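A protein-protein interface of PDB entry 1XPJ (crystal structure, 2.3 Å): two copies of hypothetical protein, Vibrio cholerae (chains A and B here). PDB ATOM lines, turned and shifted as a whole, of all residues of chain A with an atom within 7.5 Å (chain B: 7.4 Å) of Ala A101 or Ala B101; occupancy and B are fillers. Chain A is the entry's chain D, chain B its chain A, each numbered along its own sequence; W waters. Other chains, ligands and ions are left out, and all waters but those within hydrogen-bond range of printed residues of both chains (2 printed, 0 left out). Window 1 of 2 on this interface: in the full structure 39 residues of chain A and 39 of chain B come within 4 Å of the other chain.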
ATOM      1  N   GLY A  94      -1.904  -1.517   2.285  1.00  0.00           N
ATOM      2  CA  GLY A  94      -2.063  -2.628   3.213  1.00  0.00           C
ATOM      3  C   GLY A  94      -1.440  -3.934   2.757  1.00  0.00           C
ATOM      4  O   GLY A  94      -0.915  -4.027   1.638  1.00  0.00           O
ATOM      5  N   PHE A  95      -1.500  -4.949   3.622  1.00  0.00           N
ATOM      6  CA  PHE A  95      -1.023  -6.283   3.276  1.00  0.00           C
ATOM      7  C   PHE A  95      -1.435  -7.372   4.265  1.00  0.00           C
ATOM      8  O   PHE A  95      -1.986  -7.104   5.358  1.00  0.00           O
ATOM      9  CB  PHE A  95       0.500  -6.324   3.015  1.00  0.00           C
ATOM     10  CG  PHE A  95       1.358  -5.864   4.180  1.00  0.00           C
ATOM     11  CD1 PHE A  95       1.844  -6.776   5.106  1.00  0.00           C
ATOM     12  CD2 PHE A  95       1.712  -4.526   4.317  1.00  0.00           C
ATOM     13  CE1 PHE A  95       2.646  -6.361   6.181  1.00  0.00           C
ATOM     14  CE2 PHE A  95       2.519  -4.088   5.374  1.00  0.00           C
ATOM     15  CZ  PHE A  95       2.995  -5.002   6.302  1.00  0.00           C
ATOM     16  N   TYR A  96      -1.134  -8.601   3.854  1.00  0.00           N
ATOM     17  CA  TYR A  96      -1.536  -9.801   4.553  1.00  0.00           C
ATOM     18  C   TYR A  96      -0.325 -10.386   5.283  1.00  0.00           C
ATOM     19  O   TYR A  96       0.787 -10.354   4.739  1.00  0.00           O
ATOM     20  CB  TYR A  96      -2.117 -10.774   3.533  1.00  0.00           C
ATOM     21  CG  TYR A  96      -3.305 -10.191   2.781  1.00  0.00           C
ATOM     22  CD1 TYR A  96      -4.607 -10.381   3.238  1.00  0.00           C
ATOM     23  CD2 TYR A  96      -3.120  -9.421   1.622  1.00  0.00           C
ATOM     24  CE1 TYR A  96      -5.695  -9.829   2.565  1.00  0.00           C
ATOM     25  CE2 TYR A  96      -4.198  -8.864   0.951  1.00  0.00           C
ATOM     26  CZ  TYR A  96      -5.481  -9.070   1.428  1.00  0.00           C
ATOM     27  OH  TYR A  96      -6.559  -8.527   0.755  1.00  0.00           O
ATOM     28  N   ILE A  97      -0.535 -10.854   6.520  1.00  0.00           N
ATOM     29  CA  ILE A  97       0.495 -11.534   7.307  1.00  0.00           C
ATOM     30  C   ILE A  97      -0.014 -12.924   7.678  1.00  0.00           C
ATOM     31  O   ILE A  97      -1.132 -13.066   8.223  1.00  0.00           O
ATOM     32  CB  ILE A  97       0.879 -10.745   8.600  1.00  0.00           C
ATOM     33  CG1 ILE A  97       1.257  -9.296   8.267  1.00  0.00           C
ATOM     34  CG2 ILE A  97       2.024 -11.457   9.341  1.00  0.00           C
ATOM     35  CD1 ILE A  97       1.185  -8.361   9.442  1.00  0.00           C
ATOM     36  N   ASP A  98       0.813 -13.933   7.381  1.00  0.00           N
ATOM     37  CA  ASP A  98       0.416 -15.335   7.478  1.00  0.00           C
ATOM     38  C   ASP A  98       1.656 -16.242   7.456  1.00  0.00           C
ATOM     39  O   ASP A  98       2.530 -16.044   6.611  1.00  0.00           O
ATOM     40  CB  ASP A  98      -0.496 -15.662   6.291  1.00  0.00           C
ATOM     41  CG  ASP A  98      -1.203 -16.993   6.433  1.00  0.00           C
ATOM     42  OD1 ASP A  98      -0.645 -17.946   7.038  1.00  0.00           O
ATOM     43  OD2 ASP A  98      -2.342 -17.188   5.953  1.00  0.00           O
ATOM     44  N   ASP A  99       1.728 -17.230   8.354  1.00  0.00           N
ATOM     45  CA  ASP A  99       2.866 -18.166   8.391  1.00  0.00           C
ATOM     46  C   ASP A  99       2.906 -19.186   7.253  1.00  0.00           C
ATOM     47  O   ASP A  99       3.941 -19.818   7.041  1.00  0.00           O
ATOM     48  CB  ASP A  99       3.033 -18.856   9.764  1.00  0.00           C
ATOM     49  CG  ASP A  99       1.923 -19.863  10.086  1.00  0.00           C
ATOM     50  OD1 ASP A  99       0.827 -19.791   9.506  1.00  0.00           O
ATOM     51  OD2 ASP A  99       2.048 -20.762  10.935  1.00  0.00           O
ATOM     52  N   ARG A 100       1.782 -19.350   6.546  1.00  0.00           N
ATOM     53  CA  ARG A 100       1.719 -20.218   5.370  1.00  0.00           C
ATOM     54  C   ARG A 100       1.558 -19.436   4.067  1.00  0.00           C
ATOM     55  O   ARG A 100       1.025 -19.960   3.104  1.00  0.00           O
ATOM     56  CB  ARG A 100       0.599 -21.259   5.488  1.00  0.00           C
ATOM     57  CG  ARG A 100       0.591 -22.061   6.773  1.00  0.00           C
ATOM     58  CD  ARG A 100       1.508 -23.270   6.778  1.00  0.00           C
ATOM     59  NE  ARG A 100       1.161 -24.240   5.743  1.00  0.00           N
ATOM     60  CZ  ARG A 100       1.837 -25.359   5.508  1.00  0.00           C
ATOM     61  NH1 ARG A 100       2.897 -25.661   6.245  1.00  0.00           N
ATOM     62  NH2 ARG A 100       1.453 -26.180   4.537  1.00  0.00           N
ATOM     63  N   ALA A 101       2.039 -18.198   4.030  1.00  0.00           N
ATOM     64  CA  ALA A 101       1.885 -17.372   2.844  1.00  0.00           C
ATOM     65  C   ALA A 101       3.123 -17.417   1.963  1.00  0.00           C
ATOM     66  O   ALA A 101       4.235 -17.274   2.462  1.00  0.00           O
ATOM     67  CB  ALA A 101       1.610 -15.951   3.248  1.00  0.00           C
ATOM     68  N   VAL A 102       2.928 -17.619   0.660  1.00  0.00           N
ATOM     69  CA  VAL A 102       3.985 -17.373  -0.312  1.00  0.00           C
ATOM     70  C   VAL A 102       3.595 -16.339  -1.365  1.00  0.00           C
ATOM     71  O   VAL A 102       2.424 -16.201  -1.728  1.00  0.00           O
ATOM     72  CB  VAL A 102       4.547 -18.675  -1.017  1.00  0.00           C
ATOM     73  CG1 VAL A 102       4.987 -19.730   0.015  1.00  0.00           C
ATOM     74  CG2 VAL A 102       3.567 -19.242  -2.039  1.00  0.00           C
ATOM     75  N   ARG A 103       4.605 -15.608  -1.834  1.00  0.00           N
ATOM     76  CA  ARG A 103       4.447 -14.675  -2.933  1.00  0.00           C
ATOM     77  C   ARG A 103       4.528 -15.406  -4.284  1.00  0.00           C
ATOM     78  O   ARG A 103       5.233 -16.408  -4.411  1.00  0.00           O
ATOM     79  CB  ARG A 103       5.499 -13.572  -2.817  1.00  0.00           C
ATOM     80  CG  ARG A 103       5.305 -12.689  -1.567  1.00  0.00           C
ATOM     81  CD  ARG A 103       6.285 -11.495  -1.462  1.00  0.00           C
ATOM     82  NE  ARG A 103       7.638 -11.909  -1.094  1.00  0.00           N
ATOM     83  CZ  ARG A 103       8.027 -12.211   0.141  1.00  0.00           C
ATOM     84  NH1 ARG A 103       7.168 -12.146   1.150  1.00  0.00           N
ATOM     85  NH2 ARG A 103       9.283 -12.580   0.371  1.00  0.00           N
ATOM     86  N   PRO A 104       3.790 -14.923  -5.282  1.00  0.00           N
ATOM     87  CA  PRO A 104       3.704 -15.618  -6.577  1.00  0.00           C
ATOM     88  C   PRO A 104       5.058 -15.915  -7.214  1.00  0.00           C
ATOM     89  O   PRO A 104       5.182 -16.976  -7.833  1.00  0.00           O
ATOM     90  CB  PRO A 104       2.835 -14.691  -7.462  1.00  0.00           C
ATOM     91  CG  PRO A 104       2.455 -13.507  -6.640  1.00  0.00           C
ATOM     92  CD  PRO A 104       2.935 -13.721  -5.231  1.00  0.00           C
ATOM     93  N   GLU A 106       7.793 -16.606  -5.489  1.00  0.00           N
ATOM     94  CA  GLU A 106       8.367 -17.727  -4.741  1.00  0.00           C
ATOM     95  C   GLU A 106       7.705 -19.035  -5.185  1.00  0.00           C
ATOM     96  O   GLU A 106       8.383 -20.030  -5.382  1.00  0.00           O
ATOM     97  CB  GLU A 106       8.237 -17.531  -3.220  1.00  0.00           C
ATOM     98  CG  GLU A 106       8.890 -16.257  -2.675  1.00  0.00           C
ATOM     99  CD  GLU A 106       8.613 -16.033  -1.194  1.00  0.00           C
ATOM    100  OE1 GLU A 106       7.433 -15.819  -0.826  1.00  0.00           O
ATOM    101  OE2 GLU A 106       9.573 -16.071  -0.385  1.00  0.00           O
ATOM    102  N   ILE A 115       9.259 -25.034  -0.534  1.00  0.00           N
ATOM    103  CA  ILE A 115       8.168 -24.258   0.038  1.00  0.00           C
ATOM    104  C   ILE A 115       7.910 -24.746   1.468  1.00  0.00           C
ATOM    105  O   ILE A 115       7.689 -23.943   2.382  1.00  0.00           O
ATOM    106  CB  ILE A 115       6.903 -24.317  -0.847  1.00  0.00           C
ATOM    107  CG1 ILE A 115       7.045 -23.348  -2.016  1.00  0.00           C
ATOM    108  CG2 ILE A 115       5.650 -23.947  -0.055  1.00  0.00           C
ATOM    109  CD1 ILE A 115       6.081 -23.615  -3.129  1.00  0.00           C
ATOM    110  N   LEU A 118      10.520 -23.166   3.746  1.00  0.00           N
ATOM    111  CA  LEU A 118      10.203 -21.774   4.098  1.00  0.00           C
ATOM    112  C   LEU A 118       9.330 -21.722   5.348  1.00  0.00           C
ATOM    113  O   LEU A 118       9.545 -20.910   6.240  1.00  0.00           O
ATOM    114  CB  LEU A 118       9.455 -21.096   2.942  1.00  0.00           C
ATOM    115  CG  LEU A 118       9.867 -19.712   2.428  1.00  0.00           C
ATOM    116  CD1 LEU A 118      11.354 -19.623   2.099  1.00  0.00           C
ATOM    117  CD2 LEU A 118       9.021 -19.352   1.210  1.00  0.00           C
ATOM    118  N   PHE A 119       8.345 -22.615   5.386  1.00  0.00           N
ATOM    119  CA  PHE A 119       7.373 -22.694   6.463  1.00  0.00           C
ATOM    120  C   PHE A 119       7.953 -23.282   7.736  1.00  0.00           C
ATOM    121  O   PHE A 119       7.641 -22.795   8.821  1.00  0.00           O
ATOM    122  CB  PHE A 119       6.160 -23.528   6.025  1.00  0.00           C
ATOM    123  CG  PHE A 119       5.415 -22.946   4.874  1.00  0.00           C
ATOM    124  CD1 PHE A 119       4.638 -23.764   4.055  1.00  0.00           C
ATOM    125  CD2 PHE A 119       5.499 -21.583   4.589  1.00  0.00           C
ATOM    126  CE1 PHE A 119       3.949 -23.231   2.967  1.00  0.00           C
ATOM    127  CE2 PHE A 119       4.817 -21.036   3.503  1.00  0.00           C
ATOM    128  CZ  PHE A 119       4.035 -21.864   2.695  1.00  0.00           C
ATOM    129  N   GLU A 122       9.802 -20.850   9.796  1.00  0.00           N
ATOM    130  CA  GLU A 122       8.981 -20.007  10.732  1.00  0.00           C
ATOM    131  C   GLU A 122       8.672 -20.644  12.074  1.00  0.00           C
ATOM    132  O   GLU A 122       8.538 -19.966  13.080  1.00  0.00           O
ATOM    133  CB  GLU A 122       7.632 -19.914  10.048  1.00  0.00           C
ATOM    134  CG  GLU A 122       7.695 -19.002   8.870  1.00  0.00           C
ATOM    135  CD  GLU A 122       7.636 -17.649   9.448  1.00  0.00           C
ATOM    136  OE1 GLU A 122       7.145 -17.479  10.576  1.00  0.00           O
ATOM    137  OE2 GLU A 122       8.007 -16.715   8.720  1.00  0.00           O
ATOM    138  N   GLY B  94      -1.527 -27.488   2.761  1.00  0.00           N
ATOM    139  CA  GLY B  94      -1.869 -26.357   1.912  1.00  0.00           C
ATOM    140  C   GLY B  94      -1.158 -25.059   2.254  1.00  0.00           C
ATOM    141  O   GLY B  94      -0.408 -24.988   3.239  1.00  0.00           O
ATOM    142  N   PHE B  95      -1.401 -24.024   1.447  1.00  0.00           N
ATOM    143  CA  PHE B  95      -0.868 -22.684   1.728  1.00  0.00           C
ATOM    144  C   PHE B  95      -1.535 -21.598   0.890  1.00  0.00           C
ATOM    145  O   PHE B  95      -2.297 -21.879  -0.054  1.00  0.00           O
ATOM    146  CB  PHE B  95       0.674 -22.619   1.606  1.00  0.00           C
ATOM    147  CG  PHE B  95       1.241 -23.094   0.259  1.00  0.00           C
ATOM    148  CD1 PHE B  95       1.480 -22.192  -0.771  1.00  0.00           C
ATOM    149  CD2 PHE B  95       1.569 -24.420   0.057  1.00  0.00           C
ATOM    150  CE1 PHE B  95       2.012 -22.622  -2.006  1.00  0.00           C
ATOM    151  CE2 PHE B  95       2.103 -24.864  -1.152  1.00  0.00           C
ATOM    152  CZ  PHE B  95       2.336 -23.970  -2.183  1.00  0.00           C
ATOM    153  N   TYR B  96      -1.247 -20.354   1.251  1.00  0.00           N
ATOM    154  CA  TYR B  96      -1.826 -19.214   0.581  1.00  0.00           C
ATOM    155  C   TYR B  96      -0.821 -18.639  -0.405  1.00  0.00           C
ATOM    156  O   TYR B  96       0.379 -18.660  -0.127  1.00  0.00           O
ATOM    157  CB  TYR B  96      -2.275 -18.191   1.611  1.00  0.00           C
ATOM    158  CG  TYR B  96      -3.275 -18.773   2.583  1.00  0.00           C
ATOM    159  CD1 TYR B  96      -4.647 -18.553   2.419  1.00  0.00           C
ATOM    160  CD2 TYR B  96      -2.853 -19.568   3.670  1.00  0.00           C
ATOM    161  CE1 TYR B  96      -5.585 -19.103   3.309  1.00  0.00           C
ATOM    162  CE2 TYR B  96      -3.781 -20.127   4.565  1.00  0.00           C
ATOM    163  CZ  TYR B  96      -5.146 -19.889   4.376  1.00  0.00           C
ATOM    164  OH  TYR B  96      -6.073 -20.430   5.257  1.00  0.00           O
ATOM    165  N   ILE B  97      -1.308 -18.194  -1.567  1.00  0.00           N
ATOM    166  CA  ILE B  97      -0.481 -17.474  -2.548  1.00  0.00           C
ATOM    167  C   ILE B  97      -1.071 -16.073  -2.797  1.00  0.00           C
ATOM    168  O   ILE B  97      -2.261 -15.940  -3.134  1.00  0.00           O
ATOM    169  CB  ILE B  97      -0.362 -18.241  -3.898  1.00  0.00           C
ATOM    170  CG1 ILE B  97       0.129 -19.682  -3.670  1.00  0.00           C
ATOM    171  CG2 ILE B  97       0.557 -17.481  -4.872  1.00  0.00           C
ATOM    172  CD1 ILE B  97      -0.143 -20.604  -4.830  1.00  0.00           C
ATOM    173  N   ASP B  98      -0.222 -15.050  -2.648  1.00  0.00           N
ATOM    174  CA  ASP B  98      -0.656 -13.654  -2.633  1.00  0.00           C
ATOM    175  C   ASP B  98       0.533 -12.724  -2.890  1.00  0.00           C
ATOM    176  O   ASP B  98       1.561 -12.863  -2.222  1.00  0.00           O
ATOM    177  CB  ASP B  98      -1.265 -13.330  -1.258  1.00  0.00           C
ATOM    178  CG  ASP B  98      -2.151 -12.103  -1.284  1.00  0.00           C
ATOM    179  OD1 ASP B  98      -1.791 -11.095  -1.951  1.00  0.00           O
ATOM    180  OD2 ASP B  98      -3.239 -12.051  -0.651  1.00  0.00           O
ATOM    181  N   ASP B  99       0.394 -11.778  -3.824  1.00  0.00           N
ATOM    182  CA  ASP B  99       1.466 -10.819  -4.111  1.00  0.00           C
ATOM    183  C   ASP B  99       1.725  -9.798  -2.998  1.00  0.00           C
ATOM    184  O   ASP B  99       2.781  -9.172  -2.981  1.00  0.00           O
ATOM    185  CB  ASP B  99       1.291 -10.134  -5.482  1.00  0.00           C
ATOM    186  CG  ASP B  99       0.171  -9.099  -5.510  1.00  0.00           C
ATOM    187  OD1 ASP B  99      -0.732  -9.146  -4.664  1.00  0.00           O
ATOM    188  OD2 ASP B  99       0.096  -8.201  -6.369  1.00  0.00           O
ATOM    189  N   ARG B 100       0.756  -9.639  -2.086  1.00  0.00           N
ATOM    190  CA  ARG B 100       0.897  -8.773  -0.912  1.00  0.00           C
ATOM    191  C   ARG B 100       1.035  -9.565   0.390  1.00  0.00           C
ATOM    192  O   ARG B 100       0.649  -9.078   1.450  1.00  0.00           O
ATOM    193  CB  ARG B 100      -0.289  -7.809  -0.760  1.00  0.00           C
ATOM    194  CG  ARG B 100      -0.567  -6.888  -1.951  1.00  0.00           C
ATOM    195  CD  ARG B 100       0.573  -5.962  -2.336  1.00  0.00           C
ATOM    196  NE  ARG B 100       1.052  -5.160  -1.214  1.00  0.00           N
ATOM    197  CZ  ARG B 100       0.742  -3.882  -1.006  1.00  0.00           C
ATOM    198  NH1 ARG B 100      -0.064  -3.239  -1.839  1.00  0.00           N
ATOM    199  NH2 ARG B 100       1.238  -3.243   0.046  1.00  0.00           N
ATOM    200  N   ALA B 101       1.583 -10.771   0.342  1.00  0.00           N
ATOM    201  CA  ALA B 101       1.694 -11.532   1.575  1.00  0.00           C
ATOM    202  C   ALA B 101       3.103 -11.521   2.128  1.00  0.00           C
ATOM    203  O   ALA B 101       4.059 -11.689   1.388  1.00  0.00           O
ATOM    204  CB  ALA B 101       1.230 -12.933   1.376  1.00  0.00           C
ATOM    205  N   VAL B 102       3.223 -11.303   3.436  1.00  0.00           N
ATOM    206  CA  VAL B 102       4.473 -11.531   4.134  1.00  0.00           C
ATOM    207  C   VAL B 102       4.314 -12.546   5.253  1.00  0.00           C
ATOM    208  O   VAL B 102       3.263 -12.644   5.885  1.00  0.00           O
ATOM    209  CB  VAL B 102       5.128 -10.214   4.694  1.00  0.00           C
ATOM    210  CG1 VAL B 102       5.271  -9.153   3.586  1.00  0.00           C
ATOM    211  CG2 VAL B 102       4.381  -9.679   5.918  1.00  0.00           C
ATOM    212  N   ARG B 103       5.376 -13.313   5.482  1.00  0.00           N
ATOM    213  CA  ARG B 103       5.415 -14.237   6.601  1.00  0.00           C
ATOM    214  C   ARG B 103       5.740 -13.485   7.903  1.00  0.00           C
ATOM    215  O   ARG B 103       6.396 -12.446   7.854  1.00  0.00           O
ATOM    216  CB  ARG B 103       6.401 -15.368   6.310  1.00  0.00           C
ATOM    217  CG  ARG B 103       6.035 -16.167   5.043  1.00  0.00           C
ATOM    218  CD  ARG B 103       6.998 -17.330   4.709  1.00  0.00           C
ATOM    219  NE  ARG B 103       8.232 -16.884   4.065  1.00  0.00           N
ATOM    220  CZ  ARG B 103       8.326 -16.471   2.803  1.00  0.00           C
ATOM    221  NH1 ARG B 103       7.253 -16.445   2.020  1.00  0.00           N
ATOM    222  NH2 ARG B 103       9.502 -16.081   2.317  1.00  0.00           N
ATOM    223  N   PRO B 104       5.294 -13.993   9.060  1.00  0.00           N
ATOM    224  CA  PRO B 104       5.463 -13.262  10.324  1.00  0.00           C
ATOM    225  C   PRO B 104       6.926 -12.986  10.663  1.00  0.00           C
ATOM    226  O   PRO B 104       7.177 -11.974  11.321  1.00  0.00           O
ATOM    227  CB  PRO B 104       4.784 -14.166  11.372  1.00  0.00           C
ATOM    228  CG  PRO B 104       3.967 -15.133  10.601  1.00  0.00           C
ATOM    229  CD  PRO B 104       4.621 -15.288   9.268  1.00  0.00           C
ATOM    230  N   GLU B 106       9.277 -12.258   8.351  1.00  0.00           N
ATOM    231  CA  GLU B 106       9.612 -11.093   7.531  1.00  0.00           C
ATOM    232  C   GLU B 106       9.026  -9.804   8.125  1.00  0.00           C
ATOM    233  O   GLU B 106       9.694  -8.779   8.149  1.00  0.00           O
ATOM    234  CB  GLU B 106       9.121 -11.265   6.092  1.00  0.00           C
ATOM    235  CG  GLU B 106       9.713 -12.467   5.370  1.00  0.00           C
ATOM    236  CD  GLU B 106       9.102 -12.691   3.998  1.00  0.00           C
ATOM    237  OE1 GLU B 106       7.856 -12.841   3.912  1.00  0.00           O
ATOM    238  OE2 GLU B 106       9.875 -12.720   3.010  1.00  0.00           O
ATOM    239  N   ILE B 115       9.330  -3.749   3.363  1.00  0.00           N
ATOM    240  CA  ILE B 115       8.163  -4.545   2.981  1.00  0.00           C
ATOM    241  C   ILE B 115       7.683  -4.094   1.599  1.00  0.00           C
ATOM    242  O   ILE B 115       7.392  -4.919   0.724  1.00  0.00           O
ATOM    243  CB  ILE B 115       7.003  -4.417   4.020  1.00  0.00           C
ATOM    244  CG1 ILE B 115       7.436  -4.842   5.427  1.00  0.00           C
ATOM    245  CG2 ILE B 115       5.775  -5.207   3.575  1.00  0.00           C
ATOM    246  CD1 ILE B 115       7.658  -6.323   5.611  1.00  0.00           C
ATOM    247  N   LEU B 118       9.735  -5.631  -1.212  1.00  0.00           N
ATOM    248  CA  LEU B 118       9.378  -7.019  -1.538  1.00  0.00           C
ATOM    249  C   LEU B 118       8.269  -7.040  -2.571  1.00  0.00           C
ATOM    250  O   LEU B 118       8.294  -7.821  -3.510  1.00  0.00           O
ATOM    251  CB  LEU B 118       8.871  -7.776  -0.298  1.00  0.00           C
ATOM    252  CG  LEU B 118       9.821  -8.426   0.714  1.00  0.00           C
ATOM    253  CD1 LEU B 118       8.998  -9.125   1.800  1.00  0.00           C
ATOM    254  CD2 LEU B 118      10.840  -9.385   0.056  1.00  0.00           C
ATOM    255  N   PHE B 119       7.289  -6.172  -2.366  1.00  0.00           N
ATOM    256  CA  PHE B 119       6.103  -6.107  -3.199  1.00  0.00           C
ATOM    257  C   PHE B 119       6.417  -5.531  -4.566  1.00  0.00           C
ATOM    258  O   PHE B 119       5.969  -6.075  -5.574  1.00  0.00           O
ATOM    259  CB  PHE B 119       5.017  -5.273  -2.498  1.00  0.00           C
ATOM    260  CG  PHE B 119       4.547  -5.864  -1.195  1.00  0.00           C
ATOM    261  CD1 PHE B 119       4.651  -7.235  -0.956  1.00  0.00           C
ATOM    262  CD2 PHE B 119       4.017  -5.044  -0.195  1.00  0.00           C
ATOM    263  CE1 PHE B 119       4.223  -7.792   0.253  1.00  0.00           C
ATOM    264  CE2 PHE B 119       3.578  -5.584   1.015  1.00  0.00           C
ATOM    265  CZ  PHE B 119       3.681  -6.969   1.242  1.00  0.00           C
ATOM    266  N   GLU B 122       7.967  -7.734  -7.008  1.00  0.00           N
ATOM    267  CA  GLU B 122       6.987  -8.696  -7.515  1.00  0.00           C
ATOM    268  C   GLU B 122       6.362  -8.242  -8.836  1.00  0.00           C
ATOM    269  O   GLU B 122       5.801  -9.053  -9.580  1.00  0.00           O
ATOM    270  CB  GLU B 122       5.876  -8.904  -6.476  1.00  0.00           C
ATOM    271  CG  GLU B 122       6.131 -10.026  -5.471  1.00  0.00           C
ATOM    272  CD  GLU B 122       6.223 -11.413  -6.098  1.00  0.00           C
ATOM    273  OE1 GLU B 122       6.961 -12.256  -5.549  1.00  0.00           O
ATOM    274  OE2 GLU B 122       5.560 -11.669  -7.127  1.00  0.00           O
HETATM  275  O   HOH W   1      10.219 -17.582   5.847  1.00  0.00           O
HETATM  276  O   HOH W   2       9.180 -10.594  -3.183  1.00  0.00           O
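NH2 of Arg A100 sits at hydrogen-bond distance from O of Gly B94 (2.6 Å).
The backbone NH (N) of Tyr B96 is in hydrogen-bond range of the backbone carbonyl oxygen (O) of Arg A100 (3.0 Å).
The backbone carbonyl oxygen of Tyr B96 sits at hydrogen-bond distance from the backbone NH of Val A102.
N of Asp B98 sits at hydrogen-bond distance from O of Val A102 (3.0 Å).
The guanidinium group of Arg B100 lies within hydrogen-bond range of the backbone carbonyl oxygen of Gly A94 (2.8 Å).
N of Tyr A96 lies within hydrogen-bond range of O of Arg B100, at 3.0 Å.
The guanidinium group (NH1) of Arg A103 sits at hydrogen-bond distance from the backbone carbonyl oxygen (O) of Ala B101, at 3.2 Å.
The backbone NH (N) of Val B102 lies within hydrogen-bond range of the backbone carbonyl oxygen (O) of Tyr A96.
O of Val B102 lies within hydrogen-bond range of N of Asp A98.
The backbone carbonyl oxygen of Ala A101 sits at hydrogen-bond distance from the guanidinium group of Arg B103, 3.2 Å away.
The guanidinium group of Arg B103 lies within salt-bridge range of the side-chain carboxylate of Glu A106.
The side-chain carboxylate of Glu B106 lies within salt-bridge range of the guanidinium group of Arg A103, at 2.7 Å.
N of Arg B100 lies within hydrogen-bond range of OD1 of Asp B98 (2.9 Å).
NH2 of Arg B103 is in salt-bridge range of OE2 of Glu B106 (3.5 Å).
OD1 of Asp A98 is in hydrogen-bond range of N of Arg A100 (2.8 Å).
NH2 of Arg A103 is in salt-bridge range of OE2 of Glu A106, at 3.6 Å.
Among the printed residues, merely in contact across the chains: Arg A100 with Phe B95, Phe A95 with Arg B100, Glu A122 with Arg B103, Val A102 with Ile B97, Ile A97 with Val B102, Asp A98 with Tyr B96, Leu A118 with Arg B103, Arg A103 with Glu B122, Asp A98 with Arg B103, Pro A104 with Asp B98, Pro A104 with Asp B99, Asp A98 with Pro B104, Tyr A96 with Asp B98, Arg A103 with Asp B98, Asp A99 with Pro B104, Tyr A96 with Ala B101, Arg A103 with Leu B118, Ala A101 with Tyr B96, Ala A101 with Ala B101, Glu A122 with Pro B104, Phe A119 with Phe B95, Pro A104 with Glu B122, Phe A95 with Phe B119, Val A102 with Phe B95, Phe A95 with Val B102, Ile A115 with Phe B95 and Phe A95 with Ile B115.
Of the printed residues of chain B, Asp A99 touches Pro B104.
Of the printed residues of chain B, Ala A101 touches Tyr B96 (3.6 Å), Ala B101 (3.6 Å) and Arg B103 (3.2 Å).
Printed residues of chain B within 4 Å of Val A102: Phe B95, Tyr B96, Ile B97 and Asp B98.
Printed residues of chain A within 4 Å of Ile B97: Val A102.
The nearest printed residue of chain A that does not touch Ala B101 is Val A102 (4.7 Å).
The nearest printed residue of chain A that does not touch Leu B118 is Glu A106 (6.8 Å).
Printed residues of chain A that touch a printed residue of chain B: Gly A94, Phe A95, Tyr A96, Ile A97, Asp A98, Asp A99, Arg A100, Ala A101, Val A102, Arg A103, Pro A104, Glu A106, Ile A115, Leu A118, Phe A119 and Glu A122.
Hydrophobic or aromatic side chains of chain A within 4 Å of the printed part of chain B: Phe A95, Tyr A96, Ile A97, Ala A101, Val A102, Pro A104, Ile A115, Leu A118 and Phe A119.
Along chain B the printed residues that touch a printed residue of chain A span positions 94 to 122.
Among the printed residues, 39 pairs touch across the chains.
Among the printed residues, Asp or Glu carboxylates within 4 Å of a Lys or Arg side-chain nitrogen of the other chain: Arg A103 with Glu B106 (2.7 Å) and Glu A106 with Arg B103 (2.7 Å).
Gly A94 touches Arg B100, and with the chains exchanged Arg A100 touches Gly B94.
Phe A95 touches Ile B115, and with the chains exchanged Ile A115 touches Phe B95.
Phe A95 touches Phe B119, and with the chains exchanged Phe A119 touches Phe B95.
Ile A97 touches Val B102, and with the chains exchanged Val A102 touches Ile B97.
16 positions are printed for both chains.
Of the 39 pairs that touch across the chains among the printed residues, 39 have their exchanged pair printed and touching as well.
Water W1 bridges the guanidinium group of Arg B103 and the backbone carbonyl oxygen of Leu A118.
Water W2 bridges NE of Arg A103 (2.9 Å) and O of Leu B118 (2.9 Å).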
